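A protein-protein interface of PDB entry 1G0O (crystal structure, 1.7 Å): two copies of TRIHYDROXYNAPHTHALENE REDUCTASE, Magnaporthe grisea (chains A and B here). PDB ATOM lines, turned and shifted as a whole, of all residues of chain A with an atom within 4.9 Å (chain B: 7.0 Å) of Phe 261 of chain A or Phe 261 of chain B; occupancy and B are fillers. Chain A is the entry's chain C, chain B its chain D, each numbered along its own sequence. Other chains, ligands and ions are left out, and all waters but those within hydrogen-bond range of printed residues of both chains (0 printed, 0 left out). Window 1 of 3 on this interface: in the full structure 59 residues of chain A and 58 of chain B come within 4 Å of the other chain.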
ATOM      1  N   ARG A 257     -15.845  -7.015   7.861  1.00  0.00           N
ATOM      2  CA  ARG A 257     -15.513  -8.327   7.288  1.00  0.00           C
ATOM      3  C   ARG A 257     -14.745  -8.195   5.974  1.00  0.00           C
ATOM      4  O   ARG A 257     -13.744  -8.887   5.761  1.00  0.00           O
ATOM      5  CB  ARG A 257     -16.784  -9.174   7.092  1.00  0.00           C
ATOM      6  CG  ARG A 257     -17.343  -9.705   8.409  1.00  0.00           C
ATOM      7  CD  ARG A 257     -18.732 -10.287   8.260  1.00  0.00           C
ATOM      8  NE  ARG A 257     -19.204 -10.880   9.516  1.00  0.00           N
ATOM      9  CZ  ARG A 257     -20.485 -11.009   9.854  1.00  0.00           C
ATOM     10  NH1 ARG A 257     -21.442 -10.577   9.035  1.00  0.00           N
ATOM     11  NH2 ARG A 257     -20.819 -11.610  10.993  1.00  0.00           N
ATOM     12  N   VAL A 258     -15.206  -7.295   5.103  1.00  0.00           N
ATOM     13  CA  VAL A 258     -14.537  -7.071   3.825  1.00  0.00           C
ATOM     14  C   VAL A 258     -13.144  -6.466   4.057  1.00  0.00           C
ATOM     15  O   VAL A 258     -12.194  -6.799   3.348  1.00  0.00           O
ATOM     16  CB  VAL A 258     -15.364  -6.157   2.892  1.00  0.00           C
ATOM     17  CG1 VAL A 258     -14.630  -5.969   1.573  1.00  0.00           C
ATOM     18  CG2 VAL A 258     -16.753  -6.750   2.649  1.00  0.00           C
ATOM     19  N   VAL A 259     -13.025  -5.591   5.059  1.00  0.00           N
ATOM     20  CA  VAL A 259     -11.749  -4.963   5.408  1.00  0.00           C
ATOM     21  C   VAL A 259     -10.741  -6.039   5.855  1.00  0.00           C
ATOM     22  O   VAL A 259      -9.576  -6.027   5.436  1.00  0.00           O
ATOM     23  CB  VAL A 259     -11.939  -3.877   6.518  1.00  0.00           C
ATOM     24  CG1 VAL A 259     -10.590  -3.465   7.129  1.00  0.00           C
ATOM     25  CG2 VAL A 259     -12.646  -2.638   5.922  1.00  0.00           C
ATOM     26  N   CYS A 260     -11.217  -6.996   6.652  1.00  0.00           N
ATOM     27  CA  CYS A 260     -10.354  -8.075   7.126  1.00  0.00           C
ATOM     28  C   CYS A 260      -9.870  -8.941   5.978  1.00  0.00           C
ATOM     29  O   CYS A 260      -8.717  -9.364   5.971  1.00  0.00           O
ATOM     30  CB  CYS A 260     -11.056  -8.908   8.190  1.00  0.00           C
ATOM     31  SG  CYS A 260     -11.189  -7.975   9.719  1.00  0.00           S
ATOM     32  N   PHE A 261     -10.747  -9.188   5.007  1.00  0.00           N
ATOM     33  CA  PHE A 261     -10.381  -9.958   3.825  1.00  0.00           C
ATOM     34  C   PHE A 261      -9.265  -9.212   3.070  1.00  0.00           C
ATOM     35  O   PHE A 261      -8.219  -9.783   2.751  1.00  0.00           O
ATOM     36  CB  PHE A 261     -11.606 -10.141   2.914  1.00  0.00           C
ATOM     37  CG  PHE A 261     -11.265 -10.205   1.441  1.00  0.00           C
ATOM     38  CD1 PHE A 261     -10.554 -11.302   0.921  1.00  0.00           C
ATOM     39  CD2 PHE A 261     -11.614  -9.151   0.588  1.00  0.00           C
ATOM     40  CE1 PHE A 261     -10.187 -11.354  -0.435  1.00  0.00           C
ATOM     41  CE2 PHE A 261     -11.263  -9.176  -0.768  1.00  0.00           C
ATOM     42  CZ  PHE A 261     -10.542 -10.284  -1.290  1.00  0.00           C
ATOM     43  N   LEU A 262      -9.496  -7.936   2.772  1.00  0.00           N
ATOM     44  CA  LEU A 262      -8.507  -7.128   2.050  1.00  0.00           C
ATOM     45  C   LEU A 262      -7.181  -7.066   2.802  1.00  0.00           C
ATOM     46  O   LEU A 262      -6.115  -7.114   2.194  1.00  0.00           O
ATOM     47  CB  LEU A 262      -9.030  -5.699   1.806  1.00  0.00           C
ATOM     48  CG  LEU A 262     -10.181  -5.530   0.799  1.00  0.00           C
ATOM     49  CD1 LEU A 262     -10.680  -4.093   0.807  1.00  0.00           C
ATOM     50  CD2 LEU A 262      -9.702  -5.905  -0.598  1.00  0.00           C
ATOM     51  N   ALA A 263      -7.259  -7.017   4.128  1.00  0.00           N
ATOM     52  CA  ALA A 263      -6.066  -6.917   4.964  1.00  0.00           C
ATOM     53  C   ALA A 263      -5.276  -8.229   5.061  1.00  0.00           C
ATOM     54  O   ALA A 263      -4.109  -8.222   5.457  1.00  0.00           O
ATOM     55  CB  ALA A 263      -6.458  -6.415   6.364  1.00  0.00           C
ATOM     56  N   SER A 264      -5.922  -9.342   4.716  1.00  0.00           N
ATOM     57  CA  SER A 264      -5.296 -10.670   4.781  1.00  0.00           C
ATOM     58  C   SER A 264      -4.551 -11.046   3.492  1.00  0.00           C
ATOM     59  O   SER A 264      -4.596 -10.317   2.482  1.00  0.00           O
ATOM     60  CB  SER A 264      -6.365 -11.747   5.064  1.00  0.00           C
ATOM     61  OG  SER A 264      -7.136 -12.039   3.901  1.00  0.00           O
ATOM     62  N   ASP A 266      -5.422 -13.256   1.537  1.00  0.00           N
ATOM     63  CA  ASP A 266      -6.451 -13.502   0.516  1.00  0.00           C
ATOM     64  C   ASP A 266      -6.635 -12.308  -0.427  1.00  0.00           C
ATOM     65  O   ASP A 266      -7.114 -12.469  -1.550  1.00  0.00           O
ATOM     66  CB  ASP A 266      -7.806 -13.811   1.166  1.00  0.00           C
ATOM     67  CG  ASP A 266      -7.861 -15.189   1.789  1.00  0.00           C
ATOM     68  OD1 ASP A 266      -8.838 -15.479   2.504  1.00  0.00           O
ATOM     69  OD2 ASP A 266      -6.938 -15.989   1.557  1.00  0.00           O
ATOM     70  N   GLY A 267      -6.315 -11.110   0.059  1.00  0.00           N
ATOM     71  CA  GLY A 267      -6.467  -9.920  -0.760  1.00  0.00           C
ATOM     72  C   GLY A 267      -5.198  -9.538  -1.496  1.00  0.00           C
ATOM     73  O   GLY A 267      -5.146  -8.468  -2.103  1.00  0.00           O
ATOM     74  N   VAL A 270      -5.516  -8.283  -5.030  1.00  0.00           N
ATOM     75  CA  VAL A 270      -6.525  -7.238  -5.148  1.00  0.00           C
ATOM     76  C   VAL A 270      -5.850  -5.924  -4.755  1.00  0.00           C
ATOM     77  O   VAL A 270      -5.487  -5.720  -3.587  1.00  0.00           O
ATOM     78  CB  VAL A 270      -7.741  -7.467  -4.198  1.00  0.00           C
ATOM     79  CG1 VAL A 270      -8.751  -6.311  -4.335  1.00  0.00           C
ATOM     80  CG2 VAL A 270      -8.419  -8.796  -4.487  1.00  0.00           C
ATOM     81  N   SER B  24     -16.356 -16.311  10.437  1.00  0.00           N
ATOM     82  CA  SER B  24     -17.110 -15.727   9.336  1.00  0.00           C
ATOM     83  C   SER B  24     -16.465 -16.059   7.984  1.00  0.00           C
ATOM     84  O   SER B  24     -17.132 -16.050   6.950  1.00  0.00           O
ATOM     85  CB  SER B  24     -17.227 -14.214   9.538  1.00  0.00           C
ATOM     86  OG  SER B  24     -18.088 -13.643   8.570  1.00  0.00           O
ATOM     87  N   ALA B  25     -15.177 -16.397   8.009  1.00  0.00           N
ATOM     88  CA  ALA B  25     -14.454 -16.758   6.794  1.00  0.00           C
ATOM     89  C   ALA B  25     -14.505 -18.270   6.493  1.00  0.00           C
ATOM     90  O   ALA B  25     -14.103 -18.712   5.414  1.00  0.00           O
ATOM     91  CB  ALA B  25     -13.010 -16.291   6.899  1.00  0.00           C
ATOM     92  N   LEU B  27     -15.676 -22.103   5.555  1.00  0.00           N
ATOM     93  CA  LEU B  27     -16.507 -22.757   4.551  1.00  0.00           C
ATOM     94  C   LEU B  27     -16.779 -24.197   4.978  1.00  0.00           C
ATOM     95  O   LEU B  27     -17.289 -25.014   4.209  1.00  0.00           O
ATOM     96  CB  LEU B  27     -15.825 -22.719   3.184  1.00  0.00           C
ATOM     97  CG  LEU B  27     -15.657 -21.325   2.562  1.00  0.00           C
ATOM     98  CD1 LEU B  27     -14.923 -21.420   1.229  1.00  0.00           C
ATOM     99  CD2 LEU B  27     -17.030 -20.688   2.393  1.00  0.00           C
ATOM    100  N   LEU B  49     -11.232 -24.433  -2.142  1.00  0.00           N
ATOM    101  CA  LEU B  49     -12.536 -24.567  -1.497  1.00  0.00           C
ATOM    102  C   LEU B  49     -12.484 -25.841  -0.628  1.00  0.00           C
ATOM    103  O   LEU B  49     -12.970 -25.853   0.511  1.00  0.00           O
ATOM    104  CB  LEU B  49     -13.654 -24.678  -2.554  1.00  0.00           C
ATOM    105  CG  LEU B  49     -14.074 -23.396  -3.314  1.00  0.00           C
ATOM    106  CD1 LEU B  49     -14.883 -23.723  -4.581  1.00  0.00           C
ATOM    107  CD2 LEU B  49     -14.864 -22.466  -2.393  1.00  0.00           C
ATOM    108  N   ARG B  52     -10.546 -25.438   2.619  1.00  0.00           N
ATOM    109  CA  ARG B  52     -11.296 -24.657   3.590  1.00  0.00           C
ATOM    110  C   ARG B  52     -12.550 -25.353   4.143  1.00  0.00           C
ATOM    111  O   ARG B  52     -13.364 -24.735   4.841  1.00  0.00           O
ATOM    112  CB  ARG B  52     -11.608 -23.273   3.009  1.00  0.00           C
ATOM    113  CG  ARG B  52     -10.348 -22.493   2.660  1.00  0.00           C
ATOM    114  CD  ARG B  52     -10.619 -21.025   2.353  1.00  0.00           C
ATOM    115  NE  ARG B  52      -9.400 -20.379   1.868  1.00  0.00           N
ATOM    116  CZ  ARG B  52      -9.094 -19.092   2.025  1.00  0.00           C
ATOM    117  NH1 ARG B  52      -9.917 -18.271   2.659  1.00  0.00           N
ATOM    118  NH2 ARG B  52      -7.954 -18.629   1.534  1.00  0.00           N
ATOM    119  N   ARG B 158     -24.483 -18.839  -2.748  1.00  0.00           N
ATOM    120  CA  ARG B 158     -23.485 -18.019  -3.442  1.00  0.00           C
ATOM    121  C   ARG B 158     -23.285 -18.414  -4.901  1.00  0.00           C
ATOM    122  O   ARG B 158     -23.136 -19.596  -5.205  1.00  0.00           O
ATOM    123  CB  ARG B 158     -22.132 -18.164  -2.735  1.00  0.00           C
ATOM    124  CG  ARG B 158     -22.102 -17.714  -1.271  1.00  0.00           C
ATOM    125  CD  ARG B 158     -22.131 -16.202  -1.197  1.00  0.00           C
ATOM    126  NE  ARG B 158     -21.842 -15.675   0.139  1.00  0.00           N
ATOM    127  CZ  ARG B 158     -22.771 -15.319   1.020  1.00  0.00           C
ATOM    128  NH1 ARG B 158     -24.054 -15.452   0.720  1.00  0.00           N
ATOM    129  NH2 ARG B 158     -22.422 -14.730   2.157  1.00  0.00           N
ATOM    130  N   ILE B 160     -20.853 -17.274  -8.116  1.00  0.00           N
ATOM    131  CA  ILE B 160     -19.695 -16.506  -8.549  1.00  0.00           C
ATOM    132  C   ILE B 160     -19.429 -16.783 -10.023  1.00  0.00           C
ATOM    133  O   ILE B 160     -19.194 -17.914 -10.416  1.00  0.00           O
ATOM    134  CB  ILE B 160     -18.443 -16.823  -7.686  1.00  0.00           C
ATOM    135  CG1 ILE B 160     -18.710 -16.444  -6.215  1.00  0.00           C
ATOM    136  CG2 ILE B 160     -17.229 -16.038  -8.222  1.00  0.00           C
ATOM    137  CD1 ILE B 160     -18.577 -17.552  -5.223  1.00  0.00           C
ATOM    138  N   ILE B 255      -6.844 -16.070  -7.488  1.00  0.00           N
ATOM    139  CA  ILE B 255      -8.271 -16.008  -7.808  1.00  0.00           C
ATOM    140  C   ILE B 255      -9.085 -16.869  -6.845  1.00  0.00           C
ATOM    141  O   ILE B 255     -10.125 -16.441  -6.340  1.00  0.00           O
ATOM    142  CB  ILE B 255      -8.551 -16.479  -9.281  1.00  0.00           C
ATOM    143  CG1 ILE B 255      -7.611 -15.772 -10.273  1.00  0.00           C
ATOM    144  CG2 ILE B 255     -10.015 -16.244  -9.651  1.00  0.00           C
ATOM    145  CD1 ILE B 255      -7.593 -14.262 -10.163  1.00  0.00           C
ATOM    146  N   ALA B 256      -8.599 -18.076  -6.576  1.00  0.00           N
ATOM    147  CA  ALA B 256      -9.290 -18.989  -5.679  1.00  0.00           C
ATOM    148  C   ALA B 256      -9.518 -18.392  -4.283  1.00  0.00           C
ATOM    149  O   ALA B 256     -10.566 -18.626  -3.668  1.00  0.00           O
ATOM    150  CB  ALA B 256      -8.522 -20.292  -5.579  1.00  0.00           C
ATOM    151  N   ARG B 257      -8.551 -17.613  -3.798  1.00  0.00           N
ATOM    152  CA  ARG B 257      -8.660 -16.982  -2.479  1.00  0.00           C
ATOM    153  C   ARG B 257      -9.816 -15.975  -2.414  1.00  0.00           C
ATOM    154  O   ARG B 257     -10.573 -15.936  -1.436  1.00  0.00           O
ATOM    155  CB  ARG B 257      -7.343 -16.300  -2.115  1.00  0.00           C
ATOM    156  CG  ARG B 257      -6.250 -17.294  -1.743  1.00  0.00           C
ATOM    157  CD  ARG B 257      -4.873 -16.655  -1.717  1.00  0.00           C
ATOM    158  NE  ARG B 257      -3.879 -17.590  -1.201  1.00  0.00           N
ATOM    159  CZ  ARG B 257      -2.562 -17.463  -1.361  1.00  0.00           C
ATOM    160  NH1 ARG B 257      -2.057 -16.442  -2.034  1.00  0.00           N
ATOM    161  NH2 ARG B 257      -1.748 -18.357  -0.809  1.00  0.00           N
ATOM    162  N   VAL B 258      -9.948 -15.166  -3.467  1.00  0.00           N
ATOM    163  CA  VAL B 258     -11.018 -14.177  -3.544  1.00  0.00           C
ATOM    164  C   VAL B 258     -12.371 -14.888  -3.671  1.00  0.00           C
ATOM    165  O   VAL B 258     -13.353 -14.469  -3.063  1.00  0.00           O
ATOM    166  CB  VAL B 258     -10.799 -13.187  -4.719  1.00  0.00           C
ATOM    167  CG1 VAL B 258     -11.949 -12.173  -4.772  1.00  0.00           C
ATOM    168  CG2 VAL B 258      -9.459 -12.458  -4.544  1.00  0.00           C
ATOM    169  N   VAL B 259     -12.408 -15.990  -4.419  1.00  0.00           N
ATOM    170  CA  VAL B 259     -13.640 -16.758  -4.579  1.00  0.00           C
ATOM    171  C   VAL B 259     -14.094 -17.296  -3.210  1.00  0.00           C
ATOM    172  O   VAL B 259     -15.283 -17.244  -2.883  1.00  0.00           O
ATOM    173  CB  VAL B 259     -13.431 -17.906  -5.599  1.00  0.00           C
ATOM    174  CG1 VAL B 259     -14.537 -18.948  -5.500  1.00  0.00           C
ATOM    175  CG2 VAL B 259     -13.381 -17.320  -7.003  1.00  0.00           C
ATOM    176  N   CYS B 260     -13.143 -17.787  -2.412  1.00  0.00           N
ATOM    177  CA  CYS B 260     -13.458 -18.305  -1.078  1.00  0.00           C
ATOM    178  C   CYS B 260     -13.992 -17.184  -0.174  1.00  0.00           C
ATOM    179  O   CYS B 260     -14.900 -17.413   0.635  1.00  0.00           O
ATOM    180  CB  CYS B 260     -12.237 -18.981  -0.456  1.00  0.00           C
ATOM    181  SG  CYS B 260     -11.830 -20.601  -1.192  1.00  0.00           S
ATOM    182  N   PHE B 261     -13.444 -15.977  -0.318  1.00  0.00           N
ATOM    183  CA  PHE B 261     -13.924 -14.830   0.465  1.00  0.00           C
ATOM    184  C   PHE B 261     -15.398 -14.568   0.100  1.00  0.00           C
ATOM    185  O   PHE B 261     -16.261 -14.507   0.976  1.00  0.00           O
ATOM    186  CB  PHE B 261     -13.072 -13.574   0.176  1.00  0.00           C
ATOM    187  CG  PHE B 261     -13.838 -12.258   0.275  1.00  0.00           C
ATOM    188  CD1 PHE B 261     -14.332 -11.801   1.510  1.00  0.00           C
ATOM    189  CD2 PHE B 261     -14.066 -11.479  -0.874  1.00  0.00           C
ATOM    190  CE1 PHE B 261     -15.045 -10.588   1.603  1.00  0.00           C
ATOM    191  CE2 PHE B 261     -14.768 -10.275  -0.806  1.00  0.00           C
ATOM    192  CZ  PHE B 261     -15.265  -9.818   0.438  1.00  0.00           C
ATOM    193  N   LEU B 262     -15.678 -14.443  -1.197  1.00  0.00           N
ATOM    194  CA  LEU B 262     -17.040 -14.172  -1.668  1.00  0.00           C
ATOM    195  C   LEU B 262     -18.005 -15.276  -1.276  1.00  0.00           C
ATOM    196  O   LEU B 262     -19.157 -15.009  -0.956  1.00  0.00           O
ATOM    197  CB  LEU B 262     -17.064 -13.999  -3.186  1.00  0.00           C
ATOM    198  CG  LEU B 262     -16.384 -12.763  -3.771  1.00  0.00           C
ATOM    199  CD1 LEU B 262     -16.323 -12.913  -5.298  1.00  0.00           C
ATOM    200  CD2 LEU B 262     -17.151 -11.510  -3.375  1.00  0.00           C
ATOM    201  N   ALA B 263     -17.519 -16.515  -1.298  1.00  0.00           N
ATOM    202  CA  ALA B 263     -18.329 -17.684  -0.949  1.00  0.00           C
ATOM    203  C   ALA B 263     -18.637 -17.790   0.557  1.00  0.00           C
ATOM    204  O   ALA B 263     -19.592 -18.464   0.946  1.00  0.00           O
ATOM    205  CB  ALA B 263     -17.637 -18.970  -1.441  1.00  0.00           C
ATOM    206  N   SER B 264     -17.843 -17.117   1.388  1.00  0.00           N
ATOM    207  CA  SER B 264     -18.013 -17.149   2.847  1.00  0.00           C
ATOM    208  C   SER B 264     -18.979 -16.079   3.350  1.00  0.00           C
ATOM    209  O   SER B 264     -19.470 -15.248   2.560  1.00  0.00           O
ATOM    210  CB  SER B 264     -16.663 -16.948   3.536  1.00  0.00           C
ATOM    211  OG  SER B 264     -16.267 -15.594   3.458  1.00  0.00           O
ATOM    212  N   ASN B 265     -19.227 -16.090   4.665  1.00  0.00           N
ATOM    213  CA  ASN B 265     -20.111 -15.106   5.279  1.00  0.00           C
ATOM    214  C   ASN B 265     -19.531 -13.681   5.187  1.00  0.00           C
ATOM    215  O   ASN B 265     -20.267 -12.686   5.255  1.00  0.00           O
ATOM    216  CB  ASN B 265     -20.399 -15.463   6.737  1.00  0.00           C
ATOM    217  CG  ASN B 265     -21.477 -14.578   7.348  1.00  0.00           C
ATOM    218  OD1 ASN B 265     -22.604 -14.507   6.839  1.00  0.00           O
ATOM    219  ND2 ASN B 265     -21.134 -13.888   8.430  1.00  0.00           N
ATOM    220  N   ASP B 266     -18.209 -13.589   5.031  1.00  0.00           N
ATOM    221  CA  ASP B 266     -17.539 -12.302   4.905  1.00  0.00           C
ATOM    222  C   ASP B 266     -18.031 -11.560   3.666  1.00  0.00           C
ATOM    223  O   ASP B 266     -17.962 -10.327   3.606  1.00  0.00           O
ATOM    224  CB  ASP B 266     -16.015 -12.490   4.809  1.00  0.00           C
ATOM    225  CG  ASP B 266     -15.378 -12.876   6.145  1.00  0.00           C
ATOM    226  OD1 ASP B 266     -14.214 -13.359   6.141  1.00  0.00           O
ATOM    227  OD2 ASP B 266     -16.034 -12.681   7.195  1.00  0.00           O
ATOM    228  N   GLY B 267     -18.497 -12.318   2.672  1.00  0.00           N
ATOM    229  CA  GLY B 267     -18.981 -11.710   1.443  1.00  0.00           C
ATOM    230  C   GLY B 267     -20.473 -11.422   1.421  1.00  0.00           C
ATOM    231  O   GLY B 267     -21.016 -11.057   0.375  1.00  0.00           O
ATOM    232  N   GLY B 268     -21.118 -11.536   2.580  1.00  0.00           N
ATOM    233  CA  GLY B 268     -22.558 -11.343   2.685  1.00  0.00           C
ATOM    234  C   GLY B 268     -23.165 -10.056   2.160  1.00  0.00           C
ATOM    235  O   GLY B 268     -24.278 -10.065   1.609  1.00  0.00           O
ATOM    236  N   VAL B 270     -21.610  -8.144  -0.115  1.00  0.00           N
ATOM    237  CA  VAL B 270     -21.042  -7.894  -1.440  1.00  0.00           C
ATOM    238  C   VAL B 270     -21.905  -8.644  -2.458  1.00  0.00           C
ATOM    239  O   VAL B 270     -21.892  -9.869  -2.494  1.00  0.00           O
ATOM    240  CB  VAL B 270     -19.571  -8.406  -1.544  1.00  0.00           C
ATOM    241  CG1 VAL B 270     -19.016  -8.181  -2.963  1.00  0.00           C
ATOM    242  CG2 VAL B 270     -18.685  -7.704  -0.505  1.00  0.00           C
ATOM    243  N   ILE B 275     -15.355  -7.840  -9.127  1.00  0.00           N
ATOM    244  CA  ILE B 275     -14.132  -7.799  -8.324  1.00  0.00           C
ATOM    245  C   ILE B 275     -12.913  -8.062  -9.209  1.00  0.00           C
ATOM    246  O   ILE B 275     -12.682  -9.200  -9.620  1.00  0.00           O
ATOM    247  CB  ILE B 275     -14.147  -8.866  -7.169  1.00  0.00           C
ATOM    248  CG1 ILE B 275     -15.477  -8.829  -6.379  1.00  0.00           C
ATOM    249  CG2 ILE B 275     -12.938  -8.658  -6.254  1.00  0.00           C
ATOM    250  CD1 ILE B 275     -15.837  -7.475  -5.777  1.00  0.00           C
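Arg 257 of chain A touches Asp 266 of chain B, and with the chains exchanged Asp 266 of chain A touches Arg 257 of chain B.
Val 258 of chain A touches Asp 266 of chain B, and with the chains exchanged Asp 266 of chain A touches Val 258 of chain B.
Val 258 of chain A touches Val 270 of chain B, and with the chains exchanged Val 270 of chain A touches Val 258 of chain B.
Phe 261 of chain B touches its own counterpart, Phe 261 of chain A.
11 positions are printed for both chains.
Hydrophobic or aromatic side chains of chain A that line the printed part of chain B: Val 258, Phe 261 and Val 270.
Along chain A the printed residues that touch a printed residue of chain B span positions 257 to 270.
Printed residues of chain B that touch a printed residue of chain A: Ser 24, Arg 52, Arg 257, Val 258, Phe 261, Asn 265, Asp 266 and Val 270.
Hydrophobic or aromatic side chains of chain B that line the printed part of chain A: Val 258, Phe 261 and Val 270.
Among the printed residues, Asp or Glu carboxylates within 4 Å of a Lys or Arg side-chain nitrogen of the other chain: Asp 266 of chain A with Arg 52 of chain B.
Arg 257 of chain A touches Asp 266 of chain B (CG to OD2, 3.5 Å).
Asp 266 of chain B touches Val 258 of chain A (O to CG2, 3.9 Å).
CG2 of Val 258 of chain A touches CG2 of Val 270 of chain B, at 3.8 Å.
Phe 261 of chain B touches Phe 261 of chain A (CD1 to CG, 3.5 Å).
CG of Arg 257 of chain B touches OD2 of Asp 266 of chain A, 3.6 Å away.
CG2 of Val 258 of chain B touches O of Asp 266 of chain A, at 3.8 Å.
CG2 of Val 270 of chain A touches CG2 of Val 258 of chain B (3.8 Å).
Phe 261 of chain A touches just one residue of chain B: Phe 261 (3.5 Å).
Phe 261 of chain B touches just one residue of chain A: Phe 261 (3.5 Å).
Of the printed residues of chain B, Asp 266 of chain A touches Arg 52 (2.8 Å), Arg 257 (3.6 Å) and Val 258 (3.8 Å).
Of the printed residues of chain B, Arg 257 of chain A touches Ser 24, Asn 265 and Asp 266.
Printed residues of chain A within 4 Å of Arg 52 of chain B: Asp 266.
Of the printed residues of chain A, Val 270 of chain B touches Val 258.
Ala 263 of chain B touches none of the printed residues of chain A.
Cys 260 of chain B touches none of the printed residues of chain A.
The backbone carbonyl oxygen of Phe 261 of chain A lies within hydrogen-bond range of the side-chain hydroxyl of Ser 264 of chain A, at 2.8 Å.
The backbone NH (N) of Asp 266 of chain A lies close to the side-chain hydroxyl (OG) of Ser 264 of chain A (3.2 Å).
The side-chain hydroxyl (OG) of Ser 24 of chain B is in hydrogen-bond range of the side-chain amide nitrogen (ND2) of Asn 265 of chain B (3.1 Å).
The side-chain carboxylate (OD2) of Asp 266 of chain B is in hydrogen-bond range of the side-chain hydroxyl (OG) of Ser 24 of chain B (2.7 Å).
The side-chain hydroxyl of Ser 264 of chain B sits at hydrogen-bond distance from the backbone carbonyl oxygen of Phe 261 of chain B, 2.7 Å away.
The side-chain hydroxyl (OG) of Ser 264 of chain B lies close to the backbone NH (N) of Asp 266 of chain B (3.2 Å).
The side-chain hydroxyl of Ser 24 of chain B lies within hydrogen-bond range of the guanidinium group of Arg 257 of chain A (3.1 Å).
NH1 of Arg 257 of chain A lies close to ND2 of Asn 265 of chain B (3.4 Å).
The side-chain carboxylate of Asp 266 of chain A is in salt-bridge range of the guanidinium group of Arg 52 of chain B (2.8 Å).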
